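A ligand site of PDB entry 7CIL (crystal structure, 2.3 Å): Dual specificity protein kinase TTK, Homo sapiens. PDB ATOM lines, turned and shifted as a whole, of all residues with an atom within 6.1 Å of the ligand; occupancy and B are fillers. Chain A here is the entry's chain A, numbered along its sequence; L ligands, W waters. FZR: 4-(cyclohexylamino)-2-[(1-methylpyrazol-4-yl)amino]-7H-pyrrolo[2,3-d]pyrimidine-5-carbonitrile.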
ATOM      1  N   LYS A  15     -11.846 -19.863  10.123  1.00  0.00           N
ATOM      2  CA  LYS A  15     -11.583 -20.423   8.807  1.00  0.00           C
ATOM      3  C   LYS A  15     -10.982 -21.810   8.967  1.00  0.00           C
ATOM      4  O   LYS A  15     -10.405 -22.131  10.001  1.00  0.00           O
ATOM      5  CB  LYS A  15     -10.651 -19.500   8.006  1.00  0.00           C
ATOM      6  CG  LYS A  15      -9.744 -20.164   6.970  1.00  0.00           C
ATOM      7  CD  LYS A  15      -8.601 -19.253   6.550  1.00  0.00           C
ATOM      8  CE  LYS A  15      -7.923 -18.657   7.765  1.00  0.00           C
ATOM      9  NZ  LYS A  15      -6.584 -18.060   7.447  1.00  0.00           N
ATOM     10  N   ILE A  17      -8.043 -24.055   7.988  1.00  0.00           N
ATOM     11  CA  ILE A  17      -6.692 -23.965   7.483  1.00  0.00           C
ATOM     12  C   ILE A  17      -6.398 -25.108   6.524  1.00  0.00           C
ATOM     13  O   ILE A  17      -5.720 -24.933   5.498  1.00  0.00           O
ATOM     14  CB  ILE A  17      -5.708 -23.966   8.653  1.00  0.00           C
ATOM     15  CG1 ILE A  17      -5.883 -22.744   9.536  1.00  0.00           C
ATOM     16  CG2 ILE A  17      -4.283 -24.128   8.176  1.00  0.00           C
ATOM     17  CD1 ILE A  17      -5.098 -22.858  10.828  1.00  0.00           C
ATOM     18  N   GLY A  18      -6.856 -26.304   6.852  1.00  0.00           N
ATOM     19  CA  GLY A  18      -6.410 -27.445   6.068  1.00  0.00           C
ATOM     20  C   GLY A  18      -7.221 -28.673   6.399  1.00  0.00           C
ATOM     21  O   GLY A  18      -8.106 -28.654   7.264  1.00  0.00           O
ATOM     22  N   SER A  19      -6.895 -29.743   5.701  1.00  0.00           N
ATOM     23  CA  SER A  19      -7.640 -30.986   5.792  1.00  0.00           C
ATOM     24  C   SER A  19      -6.763 -32.056   5.170  1.00  0.00           C
ATOM     25  O   SER A  19      -5.809 -31.751   4.457  1.00  0.00           O
ATOM     26  CB  SER A  19      -8.989 -30.898   5.081  1.00  0.00           C
ATOM     27  OG  SER A  19      -8.805 -30.678   3.696  1.00  0.00           O
ATOM     28  N   VAL A  25      -8.304 -28.860  10.133  1.00  0.00           N
ATOM     29  CA  VAL A  25      -7.731 -27.901  11.063  1.00  0.00           C
ATOM     30  C   VAL A  25      -8.370 -26.543  10.827  1.00  0.00           C
ATOM     31  O   VAL A  25      -8.445 -26.069   9.696  1.00  0.00           O
ATOM     32  CB  VAL A  25      -6.200 -27.760  10.937  1.00  0.00           C
ATOM     33  CG1 VAL A  25      -5.678 -26.840  12.037  1.00  0.00           C
ATOM     34  CG2 VAL A  25      -5.532 -29.077  11.033  1.00  0.00           C
ATOM     35  N   GLN A  27      -8.803 -22.383  12.232  1.00  0.00           N
ATOM     36  CA  GLN A  27      -8.355 -21.218  12.959  1.00  0.00           C
ATOM     37  C   GLN A  27      -9.532 -20.730  13.792  1.00  0.00           C
ATOM     38  O   GLN A  27     -10.636 -20.563  13.251  1.00  0.00           O
ATOM     39  CB  GLN A  27      -7.902 -20.172  11.957  1.00  0.00           C
ATOM     40  CG  GLN A  27      -6.896 -19.177  12.375  1.00  0.00           C
ATOM     41  CD  GLN A  27      -6.748 -18.125  11.277  1.00  0.00           C
ATOM     42  OE1 GLN A  27      -7.731 -17.716  10.671  1.00  0.00           O
ATOM     43  NE2 GLN A  27      -5.525 -17.707  11.014  1.00  0.00           N
ATOM     44  N   ALA A  37      -5.476 -22.895  16.972  1.00  0.00           N
ATOM     45  CA  ALA A  37      -5.800 -23.831  15.918  1.00  0.00           C
ATOM     46  C   ALA A  37      -6.444 -25.054  16.565  1.00  0.00           C
ATOM     47  O   ALA A  37      -6.025 -25.473  17.647  1.00  0.00           O
ATOM     48  CB  ALA A  37      -4.569 -24.219  15.086  1.00  0.00           C
ATOM     49  N   LYS A  39      -7.505 -28.969  15.619  1.00  0.00           N
ATOM     50  CA  LYS A  39      -7.514 -30.102  14.707  1.00  0.00           C
ATOM     51  C   LYS A  39      -8.662 -31.008  15.106  1.00  0.00           C
ATOM     52  O   LYS A  39      -8.841 -31.327  16.286  1.00  0.00           O
ATOM     53  CB  LYS A  39      -6.194 -30.889  14.727  1.00  0.00           C
ATOM     54  CG  LYS A  39      -6.141 -31.968  13.621  1.00  0.00           C
ATOM     55  CD  LYS A  39      -5.157 -33.088  13.927  1.00  0.00           C
ATOM     56  CE  LYS A  39      -3.763 -32.769  13.439  1.00  0.00           C
ATOM     57  NZ  LYS A  39      -3.039 -34.027  13.015  1.00  0.00           N
ATOM     58  N   GLU A  57       0.367 -39.792  18.329  1.00  0.00           N
ATOM     59  CA  GLU A  57       0.639 -38.361  18.158  1.00  0.00           C
ATOM     60  C   GLU A  57       0.328 -37.572  19.429  1.00  0.00           C
ATOM     61  O   GLU A  57       1.138 -36.765  19.892  1.00  0.00           O
ATOM     62  CB  GLU A  57      -0.157 -37.789  16.982  1.00  0.00           C
ATOM     63  CG  GLU A  57       0.497 -36.554  16.292  1.00  0.00           C
ATOM     64  CD  GLU A  57      -0.441 -35.758  15.377  1.00  0.00           C
ATOM     65  OE1 GLU A  57      -0.172 -34.549  15.146  1.00  0.00           O
ATOM     66  OE2 GLU A  57      -1.449 -36.326  14.887  1.00  0.00           O
ATOM     67  N   ILE A  72       5.078 -27.380  18.557  1.00  0.00           N
ATOM     68  CA  ILE A  72       3.807 -26.672  18.715  1.00  0.00           C
ATOM     69  C   ILE A  72       3.105 -27.149  19.982  1.00  0.00           C
ATOM     70  O   ILE A  72       3.058 -28.354  20.265  1.00  0.00           O
ATOM     71  CB  ILE A  72       2.947 -26.872  17.463  1.00  0.00           C
ATOM     72  CG1 ILE A  72       3.479 -25.962  16.366  1.00  0.00           C
ATOM     73  CG2 ILE A  72       1.495 -26.525  17.730  1.00  0.00           C
ATOM     74  CD1 ILE A  72       2.904 -24.550  16.364  1.00  0.00           C
ATOM     75  N   MET A  88      -4.579 -26.233  19.782  1.00  0.00           N
ATOM     76  CA  MET A  88      -3.140 -26.046  19.646  1.00  0.00           C
ATOM     77  C   MET A  88      -2.792 -24.582  19.377  1.00  0.00           C
ATOM     78  O   MET A  88      -3.641 -23.747  19.026  1.00  0.00           O
ATOM     79  CB  MET A  88      -2.577 -26.916  18.515  1.00  0.00           C
ATOM     80  CG  MET A  88      -2.717 -28.420  18.793  1.00  0.00           C
ATOM     81  SD  MET A  88      -2.434 -29.402  17.324  1.00  0.00           S
ATOM     82  CE  MET A  88      -3.844 -28.939  16.357  1.00  0.00           C
ATOM     83  N   GLU A  89      -1.525 -24.304  19.619  1.00  0.00           N
ATOM     84  CA  GLU A  89      -0.867 -23.108  19.151  1.00  0.00           C
ATOM     85  C   GLU A  89      -1.145 -22.916  17.675  1.00  0.00           C
ATOM     86  O   GLU A  89      -1.059 -23.863  16.881  1.00  0.00           O
ATOM     87  CB  GLU A  89       0.638 -23.240  19.413  1.00  0.00           C
ATOM     88  CG  GLU A  89       1.410 -21.944  19.435  1.00  0.00           C
ATOM     89  CD  GLU A  89       2.870 -22.170  19.806  1.00  0.00           C
ATOM     90  OE1 GLU A  89       3.284 -23.332  19.952  1.00  0.00           O
ATOM     91  OE2 GLU A  89       3.614 -21.176  19.947  1.00  0.00           O
ATOM     92  N   CYS A  90      -1.516 -21.698  17.295  1.00  0.00           N
ATOM     93  CA  CYS A  90      -1.874 -21.444  15.909  1.00  0.00           C
ATOM     94  C   CYS A  90      -0.709 -20.700  15.256  1.00  0.00           C
ATOM     95  O   CYS A  90      -0.236 -19.682  15.777  1.00  0.00           O
ATOM     96  CB  CYS A  90      -3.171 -20.634  15.803  1.00  0.00           C
ATOM     97  SG  CYS A  90      -3.660 -20.242  14.084  1.00  0.00           S
ATOM     98  N   GLY A  91      -0.234 -21.232  14.151  1.00  0.00           N
ATOM     99  CA  GLY A  91       0.846 -20.611  13.419  1.00  0.00           C
ATOM    100  C   GLY A  91       0.331 -19.571  12.451  1.00  0.00           C
ATOM    101  O   GLY A  91      -0.808 -19.652  11.958  1.00  0.00           O
ATOM    102  N   ASN A  92       1.181 -18.573  12.185  1.00  0.00           N
ATOM    103  CA  ASN A  92       0.908 -17.605  11.130  1.00  0.00           C
ATOM    104  C   ASN A  92       0.775 -18.285   9.773  1.00  0.00           C
ATOM    105  O   ASN A  92      -0.142 -17.984   9.015  1.00  0.00           O
ATOM    106  CB  ASN A  92       1.991 -16.528  11.136  1.00  0.00           C
ATOM    107  CG  ASN A  92       2.305 -16.060  12.535  1.00  0.00           C
ATOM    108  OD1 ASN A  92       1.437 -16.101  13.412  1.00  0.00           O
ATOM    109  ND2 ASN A  92       3.532 -15.648  12.782  1.00  0.00           N
ATOM    110  N   ILE A  93       1.626 -19.288   9.515  1.00  0.00           N
ATOM    111  CA  ILE A  93       1.662 -19.941   8.205  1.00  0.00           C
ATOM    112  C   ILE A  93       2.684 -21.071   8.269  1.00  0.00           C
ATOM    113  O   ILE A  93       3.587 -21.045   9.117  1.00  0.00           O
ATOM    114  CB  ILE A  93       2.019 -18.935   7.088  1.00  0.00           C
ATOM    115  CG1 ILE A  93       1.906 -19.594   5.707  1.00  0.00           C
ATOM    116  CG2 ILE A  93       3.406 -18.326   7.339  1.00  0.00           C
ATOM    117  CD1 ILE A  93       2.349 -18.701   4.581  1.00  0.00           C
ATOM    118  N   ASP A  94       2.558 -22.055   7.398  1.00  0.00           N
ATOM    119  CA  ASP A  94       3.563 -23.109   7.344  1.00  0.00           C
ATOM    120  C   ASP A  94       4.710 -22.672   6.445  1.00  0.00           C
ATOM    121  O   ASP A  94       4.555 -21.792   5.592  1.00  0.00           O
ATOM    122  CB  ASP A  94       2.979 -24.410   6.836  1.00  0.00           C
ATOM    123  CG  ASP A  94       2.598 -24.331   5.392  1.00  0.00           C
ATOM    124  OD1 ASP A  94       1.624 -23.604   5.112  1.00  0.00           O
ATOM    125  OD2 ASP A  94       3.249 -24.976   4.534  1.00  0.00           O
ATOM    126  N   SER A  97       4.364 -22.975   2.458  1.00  0.00           N
ATOM    127  CA  SER A  97       3.621 -21.874   1.842  1.00  0.00           C
ATOM    128  C   SER A  97       4.372 -20.554   1.931  1.00  0.00           C
ATOM    129  O   SER A  97       4.254 -19.719   1.036  1.00  0.00           O
ATOM    130  CB  SER A  97       2.239 -21.748   2.489  1.00  0.00           C
ATOM    131  OG  SER A  97       1.656 -23.039   2.651  1.00  0.00           O
ATOM    132  N   ALA A 137       6.357 -28.166   5.083  1.00  0.00           N
ATOM    133  CA  ALA A 137       5.005 -28.209   5.640  1.00  0.00           C
ATOM    134  C   ALA A 137       4.958 -28.599   7.120  1.00  0.00           C
ATOM    135  O   ALA A 137       3.983 -28.261   7.800  1.00  0.00           O
ATOM    136  CB  ALA A 137       4.138 -29.206   4.857  1.00  0.00           C
ATOM    137  N   LEU A 140       5.945 -24.539  11.286  1.00  0.00           N
ATOM    138  CA  LEU A 140       5.050 -23.402  11.314  1.00  0.00           C
ATOM    139  C   LEU A 140       5.805 -22.196  11.811  1.00  0.00           C
ATOM    140  O   LEU A 140       6.651 -22.312  12.696  1.00  0.00           O
ATOM    141  CB  LEU A 140       3.875 -23.642  12.256  1.00  0.00           C
ATOM    142  CG  LEU A 140       2.977 -24.805  11.913  1.00  0.00           C
ATOM    143  CD1 LEU A 140       1.695 -24.721  12.751  1.00  0.00           C
ATOM    144  CD2 LEU A 140       2.689 -24.819  10.426  1.00  0.00           C
ATOM    145  N   ILE A 149       5.203 -29.506  13.845  1.00  0.00           N
ATOM    146  CA  ILE A 149       3.838 -29.895  14.193  1.00  0.00           C
ATOM    147  C   ILE A 149       3.582 -31.388  14.061  1.00  0.00           C
ATOM    148  O   ILE A 149       2.701 -31.918  14.746  1.00  0.00           O
ATOM    149  CB  ILE A 149       2.789 -29.133  13.365  1.00  0.00           C
ATOM    150  CG1 ILE A 149       2.943 -29.398  11.870  1.00  0.00           C
ATOM    151  CG2 ILE A 149       2.931 -27.722  13.604  1.00  0.00           C
ATOM    152  CD1 ILE A 149       2.219 -28.370  11.004  1.00  0.00           C
ATOM    153  N   ASP A 150       4.287 -32.066  13.159  1.00  0.00           N
ATOM    154  CA  ASP A 150       4.100 -33.503  13.006  1.00  0.00           C
ATOM    155  C   ASP A 150       5.299 -34.272  13.531  1.00  0.00           C
ATOM    156  O   ASP A 150       6.430 -33.775  13.546  1.00  0.00           O
ATOM    157  CB  ASP A 150       3.888 -33.900  11.553  1.00  0.00           C
ATOM    158  CG  ASP A 150       2.508 -33.610  11.098  1.00  0.00           C
ATOM    159  OD1 ASP A 150       1.833 -32.797  11.771  1.00  0.00           O
ATOM    160  OD2 ASP A 150       2.084 -34.188  10.086  1.00  0.00           O
ATOM    161  N   MET A 157      -1.595 -33.687   6.383  1.00  0.00           N
ATOM    162  CA  MET A 157      -2.649 -32.897   5.774  1.00  0.00           C
ATOM    163  C   MET A 157      -2.100 -31.862   4.816  1.00  0.00           C
ATOM    164  O   MET A 157      -0.894 -31.599   4.755  1.00  0.00           O
ATOM    165  CB  MET A 157      -3.496 -32.209   6.846  1.00  0.00           C
ATOM    166  CG  MET A 157      -4.151 -33.200   7.775  1.00  0.00           C
ATOM    167  SD  MET A 157      -4.670 -32.384   9.284  1.00  0.00           S
ATOM    168  CE  MET A 157      -5.939 -31.373   8.610  1.00  0.00           C
ATOM    169  N   GLN A 158      -3.008 -31.247   4.058  1.00  0.00           N
ATOM    170  CA  GLN A 158      -2.674 -30.257   3.056  1.00  0.00           C
ATOM    171  C   GLN A 158      -3.449 -28.971   3.301  1.00  0.00           C
ATOM    172  O   GLN A 158      -4.584 -29.023   3.810  1.00  0.00           O
ATOM    173  CB  GLN A 158      -2.968 -30.778   1.636  1.00  0.00           C
ATOM    174  CG  GLN A 158      -2.355 -32.140   1.323  1.00  0.00           C
ATOM    175  CD  GLN A 158      -0.891 -32.046   0.880  1.00  0.00           C
ATOM    176  OE1 GLN A 158      -0.309 -30.964   0.850  1.00  0.00           O
ATOM    177  NE2 GLN A 158      -0.307 -33.189   0.534  1.00  0.00           N
ATOM    178  N   PRO A 159      -2.882 -27.814   2.961  1.00  0.00           N
ATOM    179  CA  PRO A 159      -3.615 -26.554   3.109  1.00  0.00           C
ATOM    180  C   PRO A 159      -4.840 -26.543   2.200  1.00  0.00           C
ATOM    181  O   PRO A 159      -4.892 -27.214   1.168  1.00  0.00           O
ATOM    182  CB  PRO A 159      -2.606 -25.479   2.687  1.00  0.00           C
ATOM    183  CG  PRO A 159      -1.268 -26.166   2.708  1.00  0.00           C
ATOM    184  CD  PRO A 159      -1.529 -27.608   2.413  1.00  0.00           C
ATOM    185  N   ASP A 160      -5.846 -25.787   2.617  1.00  0.00           N
ATOM    186  CA  ASP A 160      -7.073 -25.681   1.822  1.00  0.00           C
ATOM    187  C   ASP A 160      -7.306 -24.250   1.351  1.00  0.00           C
ATOM    188  O   ASP A 160      -7.517 -23.351   2.154  1.00  0.00           O
ATOM    189  CB  ASP A 160      -8.271 -26.183   2.632  1.00  0.00           C
ATOM    190  CG  ASP A 160      -8.587 -27.650   2.341  1.00  0.00           C
ATOM    191  OD1 ASP A 160      -7.651 -28.415   1.997  1.00  0.00           O
ATOM    192  OD2 ASP A 160      -9.775 -28.039   2.446  1.00  0.00           O
HETATM  193  C10 FZR L   1      -1.474 -24.852  13.452  1.00  0.00           C
HETATM  194  C12 FZR L   1      -1.666 -27.066  13.490  1.00  0.00           C
HETATM  195  C19 FZR L   1      -1.635 -26.634   8.865  1.00  0.00           C
HETATM  196  C20 FZR L   1      -2.547 -27.598   8.095  1.00  0.00           C
HETATM  197  C22 FZR L   1      -0.820 -27.928   6.279  1.00  0.00           C
HETATM  198  C24 FZR L   1      -0.169 -26.853   8.512  1.00  0.00           C
HETATM  199  C17 FZR L   1      -1.674 -25.750  11.230  1.00  0.00           C
HETATM  200  C23 FZR L   1       0.134 -26.978   7.021  1.00  0.00           C
HETATM  201  C01 FZR L   1      -1.208 -22.461   6.120  1.00  0.00           C
HETATM  202  C04 FZR L   1      -1.940 -20.641   9.094  1.00  0.00           C
HETATM  203  C05 FZR L   1      -1.117 -22.650   8.571  1.00  0.00           C
HETATM  204  C06 FZR L   1      -1.457 -21.833   9.653  1.00  0.00           C
HETATM  205  C08 FZR L   1      -1.444 -23.468  11.587  1.00  0.00           C
HETATM  206  C11 FZR L   1      -1.617 -25.948  12.633  1.00  0.00           C
HETATM  207  C13 FZR L   1      -1.820 -28.510  13.064  1.00  0.00           C
HETATM  208  C15 FZR L   1      -1.551 -26.605  14.797  1.00  0.00           C
HETATM  209  C21 FZR L   1      -2.270 -27.593   6.600  1.00  0.00           C
HETATM  210  N02 FZR L   1      -1.407 -21.971   7.480  1.00  0.00           N
HETATM  211  N03 FZR L   1      -1.891 -20.770   7.775  1.00  0.00           N
HETATM  212  N07 FZR L   1      -1.344 -22.112  11.072  1.00  0.00           N
HETATM  213  N09 FZR L   1      -1.381 -23.623  12.880  1.00  0.00           N
HETATM  214  N14 FZR L   1      -1.936 -29.580  12.719  1.00  0.00           N
HETATM  215  N16 FZR L   1      -1.437 -25.257  14.752  1.00  0.00           N
HETATM  216  N18 FZR L   1      -1.813 -26.853  10.301  1.00  0.00           N
HETATM  217  N25 FZR L   1      -1.570 -24.516  10.769  1.00  0.00           N
HETATM  218  O   HOH W   1      -0.869 -32.254  12.458  1.00  0.00           O
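The backbone NH (N) of Gln 158 lies within hydrogen-bond range of the backbone carbonyl oxygen (O) of Ser 19, 2.9 Å away.
O of Ile 17 sits at hydrogen-bond distance from N of Asp 160 (3.0 Å).
The backbone carbonyl oxygen of Val 25 lies within hydrogen-bond range of the backbone NH of Ile 17 (2.7 Å).
The side-chain amino group of Lys 39 lies within salt-bridge range of the side-chain carboxylate of Glu 57 (3.4 Å).
The backbone carbonyl oxygen (O) of Ala 37 sits at hydrogen-bond distance from the backbone NH (N) of Met 88, at 2.7 Å.
OG of Ser 97 sits at hydrogen-bond distance from OD1 of Asp 94, 2.5 Å away.
N07 of the ligand lies within hydrogen-bond range of O of Gly 91 (2.7 Å).
N of Gly 91 sits at hydrogen-bond distance from N09 of the ligand (2.9 Å).
N16 of the ligand is in hydrogen-bond range of O of Glu 89, 2.6 Å away.
Water W1 lies within hydrogen-bond range of OD1 of Asp 150 (2.8 Å), NZ of Lys 39 (2.9 Å) and N14 of the ligand (2.9 Å).
Merely in contact with the ligand: Ile 17 (3.5 Å), Ala 37 (3.3 Å), Lys 39 (3.7 Å), Met 88 (3.6 Å), Cys 90 (3.8 Å), Asn 92 (3.2 Å), Ile 93 (3.7 Å), Asp 94 (3.2 Å), Leu 140 (3.2 Å), Ile 149 (3.8 Å), Met 157 (3.98 Å), Gln 158 (3.8 Å) and Pro 159 (3.7 Å).
Within 4 Å of the ligand: Ile 17, Ala 37, Lys 39, Met 88, Glu 89, Cys 90, Gly 91, Asn 92, Ile 93, Asp 94, Leu 140, Ile 149, Met 157, Gln 158 and Pro 159.
The nearest printed residue that does not touch the ligand is Val 25 (4.003 Å).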
